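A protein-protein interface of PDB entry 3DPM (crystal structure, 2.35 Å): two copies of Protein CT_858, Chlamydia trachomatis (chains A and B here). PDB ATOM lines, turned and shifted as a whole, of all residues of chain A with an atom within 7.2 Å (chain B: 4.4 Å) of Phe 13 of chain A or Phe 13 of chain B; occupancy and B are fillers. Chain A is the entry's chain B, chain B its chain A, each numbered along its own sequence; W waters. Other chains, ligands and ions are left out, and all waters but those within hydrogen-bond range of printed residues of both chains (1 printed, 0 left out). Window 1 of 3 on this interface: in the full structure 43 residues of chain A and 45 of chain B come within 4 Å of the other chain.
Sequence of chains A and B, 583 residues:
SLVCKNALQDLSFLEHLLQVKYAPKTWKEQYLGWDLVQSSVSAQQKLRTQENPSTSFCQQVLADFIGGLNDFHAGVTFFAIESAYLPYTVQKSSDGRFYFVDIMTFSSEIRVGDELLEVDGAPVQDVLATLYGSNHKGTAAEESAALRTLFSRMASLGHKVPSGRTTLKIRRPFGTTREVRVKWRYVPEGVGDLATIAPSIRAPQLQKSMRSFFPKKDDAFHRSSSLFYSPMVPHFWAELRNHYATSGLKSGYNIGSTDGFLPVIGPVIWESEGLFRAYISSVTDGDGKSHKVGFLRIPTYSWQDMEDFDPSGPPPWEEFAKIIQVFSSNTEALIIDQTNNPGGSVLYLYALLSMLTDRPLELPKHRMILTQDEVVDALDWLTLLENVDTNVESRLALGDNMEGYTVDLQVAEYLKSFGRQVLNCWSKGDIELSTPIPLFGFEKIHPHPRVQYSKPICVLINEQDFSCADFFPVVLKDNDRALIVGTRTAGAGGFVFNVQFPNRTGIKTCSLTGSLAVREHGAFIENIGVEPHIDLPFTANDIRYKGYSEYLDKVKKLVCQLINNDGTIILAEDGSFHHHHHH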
ATOM      1  N   ALA A   7      15.237 -21.069  16.119  1.00  0.00           N
ATOM      2  CA  ALA A   7      14.923 -20.894  14.704  1.00  0.00           C
ATOM      3  C   ALA A   7      14.184 -19.590  14.424  1.00  0.00           C
ATOM      4  O   ALA A   7      14.414 -18.963  13.391  1.00  0.00           O
ATOM      5  CB  ALA A   7      14.116 -22.075  14.193  1.00  0.00           C
ATOM      6  N   LEU A   8      13.302 -19.186  15.331  1.00  0.00           N
ATOM      7  CA  LEU A   8      12.551 -17.949  15.156  1.00  0.00           C
ATOM      8  C   LEU A   8      13.458 -16.736  15.298  1.00  0.00           C
ATOM      9  O   LEU A   8      13.289 -15.742  14.585  1.00  0.00           O
ATOM     10  CB  LEU A   8      11.418 -17.851  16.176  1.00  0.00           C
ATOM     11  CG  LEU A   8      10.191 -18.745  15.970  1.00  0.00           C
ATOM     12  CD1 LEU A   8       9.360 -18.783  17.258  1.00  0.00           C
ATOM     13  CD2 LEU A   8       9.370 -18.212  14.801  1.00  0.00           C
ATOM     14  N   GLN A   9      14.424 -16.827  16.210  1.00  0.00           N
ATOM     15  CA  GLN A   9      15.365 -15.740  16.445  1.00  0.00           C
ATOM     16  C   GLN A   9      16.308 -15.615  15.244  1.00  0.00           C
ATOM     17  O   GLN A   9      16.655 -14.507  14.830  1.00  0.00           O
ATOM     18  CB  GLN A   9      16.163 -16.002  17.729  1.00  0.00           C
ATOM     19  CG  GLN A   9      16.516 -14.747  18.524  1.00  0.00           C
ATOM     20  CD  GLN A   9      17.367 -13.752  17.729  1.00  0.00           C
ATOM     21  OE1 GLN A   9      18.487 -14.066  17.315  1.00  0.00           O
ATOM     22  NE2 GLN A   9      16.836 -12.548  17.515  1.00  0.00           N
ATOM     23  N   ASP A  10      16.720 -16.746  14.677  1.00  0.00           N
ATOM     24  CA  ASP A  10      17.602 -16.709  13.514  1.00  0.00           C
ATOM     25  C   ASP A  10      16.840 -16.325  12.244  1.00  0.00           C
ATOM     26  O   ASP A  10      17.395 -15.705  11.343  1.00  0.00           O
ATOM     27  CB  ASP A  10      18.327 -18.049  13.353  1.00  0.00           C
ATOM     28  CG  ASP A  10      19.308 -18.311  14.507  1.00  0.00           C
ATOM     29  OD1 ASP A  10      20.118 -17.394  14.811  1.00  0.00           O
ATOM     30  OD2 ASP A  10      19.271 -19.412  15.112  1.00  0.00           O
ATOM     31  N   LEU A  11      15.557 -16.668  12.192  1.00  0.00           N
ATOM     32  CA  LEU A  11      14.729 -16.306  11.055  1.00  0.00           C
ATOM     33  C   LEU A  11      14.665 -14.774  11.006  1.00  0.00           C
ATOM     34  O   LEU A  11      14.796 -14.175   9.934  1.00  0.00           O
ATOM     35  CB  LEU A  11      13.314 -16.853  11.222  1.00  0.00           C
ATOM     36  CG  LEU A  11      12.527 -17.237   9.967  1.00  0.00           C
ATOM     37  CD1 LEU A  11      11.053 -17.318  10.344  1.00  0.00           C
ATOM     38  CD2 LEU A  11      12.729 -16.228   8.850  1.00  0.00           C
ATOM     39  N   SER A  12      14.481 -14.140  12.166  1.00  0.00           N
ATOM     40  CA  SER A  12      14.396 -12.684  12.196  1.00  0.00           C
ATOM     41  C   SER A  12      15.706 -12.015  11.788  1.00  0.00           C
ATOM     42  O   SER A  12      15.698 -10.873  11.318  1.00  0.00           O
ATOM     43  CB  SER A  12      13.933 -12.176  13.573  1.00  0.00           C
ATOM     44  OG  SER A  12      14.597 -12.820  14.635  1.00  0.00           O
ATOM     45  N   PHE A  13      16.825 -12.720  11.947  1.00  0.00           N
ATOM     46  CA  PHE A  13      18.105 -12.145  11.545  1.00  0.00           C
ATOM     47  C   PHE A  13      18.258 -12.203  10.023  1.00  0.00           C
ATOM     48  O   PHE A  13      18.727 -11.243   9.404  1.00  0.00           O
ATOM     49  CB  PHE A  13      19.278 -12.870  12.209  1.00  0.00           C
ATOM     50  CG  PHE A  13      20.614 -12.254  11.894  1.00  0.00           C
ATOM     51  CD1 PHE A  13      20.833 -10.886  12.109  1.00  0.00           C
ATOM     52  CD2 PHE A  13      21.647 -13.024  11.358  1.00  0.00           C
ATOM     53  CE1 PHE A  13      22.062 -10.294  11.789  1.00  0.00           C
ATOM     54  CE2 PHE A  13      22.885 -12.442  11.036  1.00  0.00           C
ATOM     55  CZ  PHE A  13      23.091 -11.076  11.252  1.00  0.00           C
ATOM     56  N   LEU A  14      17.866 -13.331   9.431  1.00  0.00           N
ATOM     57  CA  LEU A  14      17.934 -13.508   7.984  1.00  0.00           C
ATOM     58  C   LEU A  14      16.996 -12.514   7.335  1.00  0.00           C
ATOM     59  O   LEU A  14      17.262 -12.014   6.238  1.00  0.00           O
ATOM     60  CB  LEU A  14      17.498 -14.913   7.586  1.00  0.00           C
ATOM     61  CG  LEU A  14      18.410 -16.071   7.981  1.00  0.00           C
ATOM     62  CD1 LEU A  14      17.797 -17.366   7.449  1.00  0.00           C
ATOM     63  CD2 LEU A  14      19.817 -15.862   7.418  1.00  0.00           C
ATOM     64  N   GLU A  15      15.884 -12.253   8.016  1.00  0.00           N
ATOM     65  CA  GLU A  15      14.886 -11.313   7.541  1.00  0.00           C
ATOM     66  C   GLU A  15      15.532  -9.944   7.538  1.00  0.00           C
ATOM     67  O   GLU A  15      15.346  -9.147   6.615  1.00  0.00           O
ATOM     68  CB  GLU A  15      13.672 -11.333   8.472  1.00  0.00           C
ATOM     69  CG  GLU A  15      12.656 -10.235   8.217  1.00  0.00           C
ATOM     70  CD  GLU A  15      11.433 -10.314   9.133  1.00  0.00           C
ATOM     71  OE1 GLU A  15      10.664  -9.329   9.168  1.00  0.00           O
ATOM     72  OE2 GLU A  15      11.228 -11.352   9.807  1.00  0.00           O
ATOM     73  N   HIS A  16      16.315  -9.688   8.579  1.00  0.00           N
ATOM     74  CA  HIS A  16      17.014  -8.422   8.718  1.00  0.00           C
ATOM     75  C   HIS A  16      18.063  -8.232   7.618  1.00  0.00           C
ATOM     76  O   HIS A  16      18.185  -7.148   7.053  1.00  0.00           O
ATOM     77  CB  HIS A  16      17.666  -8.347  10.098  1.00  0.00           C
ATOM     78  CG  HIS A  16      18.559  -7.162  10.282  1.00  0.00           C
ATOM     79  ND1 HIS A  16      19.932  -7.263  10.318  1.00  0.00           N
ATOM     80  CD2 HIS A  16      18.276  -5.845  10.418  1.00  0.00           C
ATOM     81  CE1 HIS A  16      20.459  -6.059  10.467  1.00  0.00           C
ATOM     82  NE2 HIS A  16      19.475  -5.181  10.529  1.00  0.00           N
ATOM     83  N   LEU A  17      18.814  -9.286   7.309  1.00  0.00           N
ATOM     84  CA  LEU A  17      19.842  -9.196   6.271  1.00  0.00           C
ATOM     85  C   LEU A  17      19.220  -8.787   4.935  1.00  0.00           C
ATOM     86  O   LEU A  17      19.774  -7.959   4.201  1.00  0.00           O
ATOM     87  CB  LEU A  17      20.575 -10.538   6.118  1.00  0.00           C
ATOM     88  CG  LEU A  17      21.381 -11.045   7.323  1.00  0.00           C
ATOM     89  CD1 LEU A  17      21.965 -12.417   7.006  1.00  0.00           C
ATOM     90  CD2 LEU A  17      22.491 -10.069   7.659  1.00  0.00           C
ATOM     91  N   LEU A  18      18.059  -9.363   4.631  1.00  0.00           N
ATOM     92  CA  LEU A  18      17.363  -9.052   3.389  1.00  0.00           C
ATOM     93  C   LEU A  18      16.960  -7.586   3.313  1.00  0.00           C
ATOM     94  O   LEU A  18      16.766  -7.050   2.222  1.00  0.00           O
ATOM     95  CB  LEU A  18      16.135  -9.944   3.230  1.00  0.00           C
ATOM     96  CG  LEU A  18      16.463 -11.441   3.166  1.00  0.00           C
ATOM     97  CD1 LEU A  18      15.167 -12.247   3.068  1.00  0.00           C
ATOM     98  CD2 LEU A  18      17.393 -11.723   1.980  1.00  0.00           C
ATOM     99  N   GLN A  19      16.839  -6.934   4.466  1.00  0.00           N
ATOM    100  CA  GLN A  19      16.477  -5.527   4.481  1.00  0.00           C
ATOM    101  C   GLN A  19      17.686  -4.616   4.536  1.00  0.00           C
ATOM    102  O   GLN A  19      17.540  -3.400   4.527  1.00  0.00           O
ATOM    103  CB  GLN A  19      15.560  -5.220   5.659  1.00  0.00           C
ATOM    104  CG  GLN A  19      14.138  -5.646   5.418  1.00  0.00           C
ATOM    105  CD  GLN A  19      13.280  -5.506   6.647  1.00  0.00           C
ATOM    106  OE1 GLN A  19      13.583  -6.083   7.697  1.00  0.00           O
ATOM    107  NE2 GLN A  19      12.193  -4.744   6.529  1.00  0.00           N
ATOM    108  N   VAL A  20      18.881  -5.188   4.584  1.00  0.00           N
ATOM    109  CA  VAL A  20      20.081  -4.361   4.647  1.00  0.00           C
ATOM    110  C   VAL A  20      20.970  -4.439   3.414  1.00  0.00           C
ATOM    111  O   VAL A  20      21.383  -3.406   2.883  1.00  0.00           O
ATOM    112  CB  VAL A  20      20.974  -4.733   5.848  1.00  0.00           C
ATOM    113  CG1 VAL A  20      22.150  -3.760   5.939  1.00  0.00           C
ATOM    114  CG2 VAL A  20      20.170  -4.722   7.122  1.00  0.00           C
ATOM    115  N   PHE A  65      12.466 -20.606   3.162  1.00  0.00           N
ATOM    116  CA  PHE A  65      12.272 -19.170   3.290  1.00  0.00           C
ATOM    117  C   PHE A  65      13.155 -18.443   2.274  1.00  0.00           C
ATOM    118  O   PHE A  65      12.661 -17.663   1.451  1.00  0.00           O
ATOM    119  CB  PHE A  65      12.620 -18.718   4.710  1.00  0.00           C
ATOM    120  CG  PHE A  65      12.577 -17.231   4.895  1.00  0.00           C
ATOM    121  CD1 PHE A  65      11.392 -16.529   4.712  1.00  0.00           C
ATOM    122  CD2 PHE A  65      13.727 -16.527   5.229  1.00  0.00           C
ATOM    123  CE1 PHE A  65      11.354 -15.136   4.856  1.00  0.00           C
ATOM    124  CE2 PHE A  65      13.698 -15.135   5.377  1.00  0.00           C
ATOM    125  CZ  PHE A  65      12.502 -14.443   5.187  1.00  0.00           C
ATOM    126  N   VAL A 499      27.458 -14.435   4.558  1.00  0.00           N
ATOM    127  CA  VAL A 499      27.377 -13.985   5.931  1.00  0.00           C
ATOM    128  C   VAL A 499      27.378 -15.177   6.879  1.00  0.00           C
ATOM    129  O   VAL A 499      26.612 -16.122   6.704  1.00  0.00           O
ATOM    130  CB  VAL A 499      26.085 -13.165   6.170  1.00  0.00           C
ATOM    131  CG1 VAL A 499      25.988 -12.742   7.636  1.00  0.00           C
ATOM    132  CG2 VAL A 499      26.070 -11.952   5.257  1.00  0.00           C
ATOM    133  N   GLN A 500      28.255 -15.128   7.871  1.00  0.00           N
ATOM    134  CA  GLN A 500      28.335 -16.171   8.890  1.00  0.00           C
ATOM    135  C   GLN A 500      28.051 -15.505  10.241  1.00  0.00           C
ATOM    136  O   GLN A 500      28.424 -14.350  10.466  1.00  0.00           O
ATOM    137  CB  GLN A 500      29.739 -16.805   8.949  1.00  0.00           C
ATOM    138  CG  GLN A 500      30.138 -17.685   7.760  1.00  0.00           C
ATOM    139  CD  GLN A 500      30.678 -16.891   6.579  1.00  0.00           C
ATOM    140  OE1 GLN A 500      30.981 -17.457   5.523  1.00  0.00           O
ATOM    141  NE2 GLN A 500      30.810 -15.575   6.753  1.00  0.00           N
ATOM    142  N   PHE A 501      27.388 -16.222  11.135  1.00  0.00           N
ATOM    143  CA  PHE A 501      27.119 -15.686  12.453  1.00  0.00           C
ATOM    144  C   PHE A 501      26.877 -16.847  13.394  1.00  0.00           C
ATOM    145  O   PHE A 501      26.323 -17.866  13.004  1.00  0.00           O
ATOM    146  CB  PHE A 501      25.919 -14.727  12.417  1.00  0.00           C
ATOM    147  CG  PHE A 501      24.633 -15.371  11.998  1.00  0.00           C
ATOM    148  CD1 PHE A 501      23.790 -15.950  12.941  1.00  0.00           C
ATOM    149  CD2 PHE A 501      24.262 -15.399  10.659  1.00  0.00           C
ATOM    150  CE1 PHE A 501      22.585 -16.554  12.557  1.00  0.00           C
ATOM    151  CE2 PHE A 501      23.060 -16.000  10.263  1.00  0.00           C
ATOM    152  CZ  PHE A 501      22.222 -16.578  11.219  1.00  0.00           C
ATOM    153  N   PRO A 502      27.325 -16.723  14.647  1.00  0.00           N
ATOM    154  CA  PRO A 502      27.124 -17.811  15.608  1.00  0.00           C
ATOM    155  C   PRO A 502      25.652 -18.050  15.940  1.00  0.00           C
ATOM    156  O   PRO A 502      24.890 -17.108  16.159  1.00  0.00           O
ATOM    157  CB  PRO A 502      27.939 -17.361  16.817  1.00  0.00           C
ATOM    158  CG  PRO A 502      27.896 -15.857  16.713  1.00  0.00           C
ATOM    159  CD  PRO A 502      28.080 -15.608  15.243  1.00  0.00           C
ATOM    160  N   ILE A 507      23.091 -22.905  11.239  1.00  0.00           N
ATOM    161  CA  ILE A 507      23.327 -22.133  10.024  1.00  0.00           C
ATOM    162  C   ILE A 507      24.816 -21.858   9.879  1.00  0.00           C
ATOM    163  O   ILE A 507      25.473 -21.361  10.809  1.00  0.00           O
ATOM    164  CB  ILE A 507      22.560 -20.801  10.040  1.00  0.00           C
ATOM    165  CG1 ILE A 507      21.069 -21.073  10.197  1.00  0.00           C
ATOM    166  CG2 ILE A 507      22.821 -20.027   8.762  1.00  0.00           C
ATOM    167  CD1 ILE A 507      20.260 -19.831  10.466  1.00  0.00           C
ATOM    168  N   GLN B   9      20.178  -0.817  16.601  1.00  0.00           N
ATOM    169  CA  GLN B   9      19.941  -2.112  15.974  1.00  0.00           C
ATOM    170  C   GLN B   9      21.237  -2.938  15.984  1.00  0.00           C
ATOM    171  O   GLN B   9      21.229  -4.132  16.280  1.00  0.00           O
ATOM    172  CB  GLN B   9      19.452  -1.924  14.532  1.00  0.00           C
ATOM    173  CG  GLN B   9      18.219  -2.753  14.167  1.00  0.00           C
ATOM    174  CD  GLN B   9      18.307  -4.201  14.637  1.00  0.00           C
ATOM    175  OE1 GLN B   9      19.285  -4.906  14.361  1.00  0.00           O
ATOM    176  NE2 GLN B   9      17.277  -4.652  15.345  1.00  0.00           N
ATOM    177  N   ASP B  10      22.355  -2.299  15.672  1.00  0.00           N
ATOM    178  CA  ASP B  10      23.619  -3.017  15.658  1.00  0.00           C
ATOM    179  C   ASP B  10      24.122  -3.340  17.072  1.00  0.00           C
ATOM    180  O   ASP B  10      24.783  -4.364  17.291  1.00  0.00           O
ATOM    181  CB  ASP B  10      24.640  -2.238  14.824  1.00  0.00           C
ATOM    182  CG  ASP B  10      24.242  -2.185  13.335  1.00  0.00           C
ATOM    183  OD1 ASP B  10      23.873  -3.248  12.781  1.00  0.00           O
ATOM    184  OD2 ASP B  10      24.288  -1.097  12.715  1.00  0.00           O
ATOM    185  N   LEU B  11      23.771  -2.486  18.030  1.00  0.00           N
ATOM    186  CA  LEU B  11      24.146  -2.710  19.423  1.00  0.00           C
ATOM    187  C   LEU B  11      23.393  -3.963  19.880  1.00  0.00           C
ATOM    188  O   LEU B  11      23.950  -4.828  20.553  1.00  0.00           O
ATOM    189  CB  LEU B  11      23.713  -1.526  20.300  1.00  0.00           C
ATOM    190  CG  LEU B  11      24.335  -1.292  21.691  1.00  0.00           C
ATOM    191  CD1 LEU B  11      23.262  -0.764  22.633  1.00  0.00           C
ATOM    192  CD2 LEU B  11      24.937  -2.560  22.250  1.00  0.00           C
ATOM    193  N   SER B  12      22.123  -4.059  19.499  1.00  0.00           N
ATOM    194  CA  SER B  12      21.325  -5.206  19.902  1.00  0.00           C
ATOM    195  C   SER B  12      21.893  -6.495  19.325  1.00  0.00           C
ATOM    196  O   SER B  12      21.766  -7.549  19.947  1.00  0.00           O
ATOM    197  CB  SER B  12      19.852  -5.037  19.495  1.00  0.00           C
ATOM    198  OG  SER B  12      19.662  -5.235  18.108  1.00  0.00           O
ATOM    199  N   PHE B  13      22.523  -6.426  18.152  1.00  0.00           N
ATOM    200  CA  PHE B  13      23.106  -7.632  17.582  1.00  0.00           C
ATOM    201  C   PHE B  13      24.385  -7.999  18.339  1.00  0.00           C
ATOM    202  O   PHE B  13      24.684  -9.171  18.533  1.00  0.00           O
ATOM    203  CB  PHE B  13      23.421  -7.467  16.097  1.00  0.00           C
ATOM    204  CG  PHE B  13      23.927  -8.732  15.455  1.00  0.00           C
ATOM    205  CD1 PHE B  13      23.101  -9.854  15.357  1.00  0.00           C
ATOM    206  CD2 PHE B  13      25.244  -8.837  15.026  1.00  0.00           C
ATOM    207  CE1 PHE B  13      23.582 -11.066  14.847  1.00  0.00           C
ATOM    208  CE2 PHE B  13      25.736 -10.053  14.511  1.00  0.00           C
ATOM    209  CZ  PHE B  13      24.897 -11.165  14.426  1.00  0.00           C
ATOM    210  N   LEU B  14      25.148  -7.001  18.767  1.00  0.00           N
ATOM    211  CA  LEU B  14      26.359  -7.296  19.529  1.00  0.00           C
ATOM    212  C   LEU B  14      25.950  -7.937  20.848  1.00  0.00           C
ATOM    213  O   LEU B  14      26.551  -8.901  21.292  1.00  0.00           O
ATOM    214  CB  LEU B  14      27.159  -6.026  19.820  1.00  0.00           C
ATOM    215  CG  LEU B  14      27.866  -5.329  18.655  1.00  0.00           C
ATOM    216  CD1 LEU B  14      28.702  -4.193  19.233  1.00  0.00           C
ATOM    217  CD2 LEU B  14      28.756  -6.307  17.881  1.00  0.00           C
ATOM    218  N   GLU B  15      24.921  -7.374  21.468  1.00  0.00           N
ATOM    219  CA  GLU B  15      24.384  -7.865  22.732  1.00  0.00           C
ATOM    220  C   GLU B  15      23.986  -9.337  22.601  1.00  0.00           C
ATOM    221  O   GLU B  15      24.246 -10.148  23.484  1.00  0.00           O
ATOM    222  CB  GLU B  15      23.165  -7.013  23.118  1.00  0.00           C
ATOM    223  CG  GLU B  15      22.289  -7.582  24.218  1.00  0.00           C
ATOM    224  CD  GLU B  15      21.133  -6.656  24.588  1.00  0.00           C
ATOM    225  OE1 GLU B  15      20.311  -7.045  25.450  1.00  0.00           O
ATOM    226  OE2 GLU B  15      21.050  -5.543  24.021  1.00  0.00           O
ATOM    227  N   HIS B  16      23.359  -9.673  21.483  1.00  0.00           N
ATOM    228  CA  HIS B  16      22.931 -11.033  21.232  1.00  0.00           C
ATOM    229  C   HIS B  16      24.126 -11.973  21.060  1.00  0.00           C
ATOM    230  O   HIS B  16      24.107 -13.100  21.556  1.00  0.00           O
ATOM    231  CB  HIS B  16      22.027 -11.047  20.001  1.00  0.00           C
ATOM    232  CG  HIS B  16      21.628 -12.418  19.558  1.00  0.00           C
ATOM    233  ND1 HIS B  16      22.306 -13.108  18.576  1.00  0.00           N
ATOM    234  CD2 HIS B  16      20.629 -13.233  19.970  1.00  0.00           C
ATOM    235  CE1 HIS B  16      21.739 -14.287  18.399  1.00  0.00           C
ATOM    236  NE2 HIS B  16      20.720 -14.388  19.232  1.00  0.00           N
ATOM    237  N   LEU B  17      25.164 -11.504  20.371  1.00  0.00           N
ATOM    238  CA  LEU B  17      26.371 -12.302  20.152  1.00  0.00           C
ATOM    239  C   LEU B  17      27.023 -12.716  21.463  1.00  0.00           C
ATOM    240  O   LEU B  17      27.634 -13.784  21.554  1.00  0.00           O
ATOM    241  CB  LEU B  17      27.395 -11.521  19.330  1.00  0.00           C
ATOM    242  CG  LEU B  17      27.122 -11.318  17.837  1.00  0.00           C
ATOM    243  CD1 LEU B  17      28.243 -10.488  17.235  1.00  0.00           C
ATOM    244  CD2 LEU B  17      27.018 -12.667  17.139  1.00  0.00           C
ATOM    245  N   PHE B 501      29.218  -8.735   9.700  1.00  0.00           N
ATOM    246  CA  PHE B 501      27.846  -8.683   9.215  1.00  0.00           C
ATOM    247  C   PHE B 501      27.582  -7.341   8.545  1.00  0.00           C
ATOM    248  O   PHE B 501      28.159  -6.324   8.919  1.00  0.00           O
ATOM    249  CB  PHE B 501      26.848  -8.950  10.359  1.00  0.00           C
ATOM    250  CG  PHE B 501      26.903  -7.949  11.480  1.00  0.00           C
ATOM    251  CD1 PHE B 501      25.937  -6.952  11.585  1.00  0.00           C
ATOM    252  CD2 PHE B 501      27.908  -8.008  12.440  1.00  0.00           C
ATOM    253  CE1 PHE B 501      25.969  -6.026  12.631  1.00  0.00           C
ATOM    254  CE2 PHE B 501      27.951  -7.087  13.491  1.00  0.00           C
ATOM    255  CZ  PHE B 501      26.979  -6.093  13.586  1.00  0.00           C
HETATM  256  O   HOH W   1      19.070 -16.606  18.943  1.00  0.00           O
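Phe 13 of chain A touches just one residue of chain B: Phe 13. Of the printed residues of chain B, Pro 502 of chain A touches Leu 17. Phe 13 of chain B touches just one residue of chain A: Phe 13 (3.5 Å). Of the printed residues of chain A, His 16 of chain B touches Gln 9. Of the printed residues of chain A, Leu 17 of chain B touches Pro 502 (3.3 Å).
Hydrophobic or aromatic side chains of chain B within 4 Å of the printed part of chain A: Phe 13, His 16 and Leu 17. Along chain B the printed residues that touch a printed residue of chain A span positions 9 to 17. Among the printed residues, 4 pairs touch across the chains. Among the printed residues, no Asp or Glu carboxylate lies within 4 Å of a Lys or Arg side-chain nitrogen of the other chain.
Gln 9 of chain A touches His 16 of chain B, and with the chains exchanged His 16 of chain A touches Gln 9 of chain B. Phe 13 of chain A touches its own counterpart, Phe 13 of chain B. Positions printed for both chains: 9, 10, 11, 12, 13, 14, 15, 16, 17 and 501. Of the 4 pairs that touch across the chains among the printed residues, 3 have their exchanged pair printed and touching as well.
Phe 13 of chain B touches Phe 13 of chain A. Gln 9 of chain B touches His 16 of chain A (OE1 to NE2, 3.8 Å). Pro 502 of chain A touches Leu 17 of chain B.
Water W1 bridges NE2 of His 16 of chain B and OE1 of Gln 9 of chain A.
O of Gln 9 of chain B lies within hydrogen-bond range of OG of Ser 12 of chain B (2.6 Å). The backbone carbonyl oxygen (O) of Gln 9 of chain A lies within hydrogen-bond range of the side-chain hydroxyl (OG) of Ser 12 of chain A (2.7 Å).
A ring nitrogen (NE2) of His 16 of chain B is in hydrogen-bond range of the side-chain amide oxygen (OE1) of Gln 9 of chain A, 3.0 Å away.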
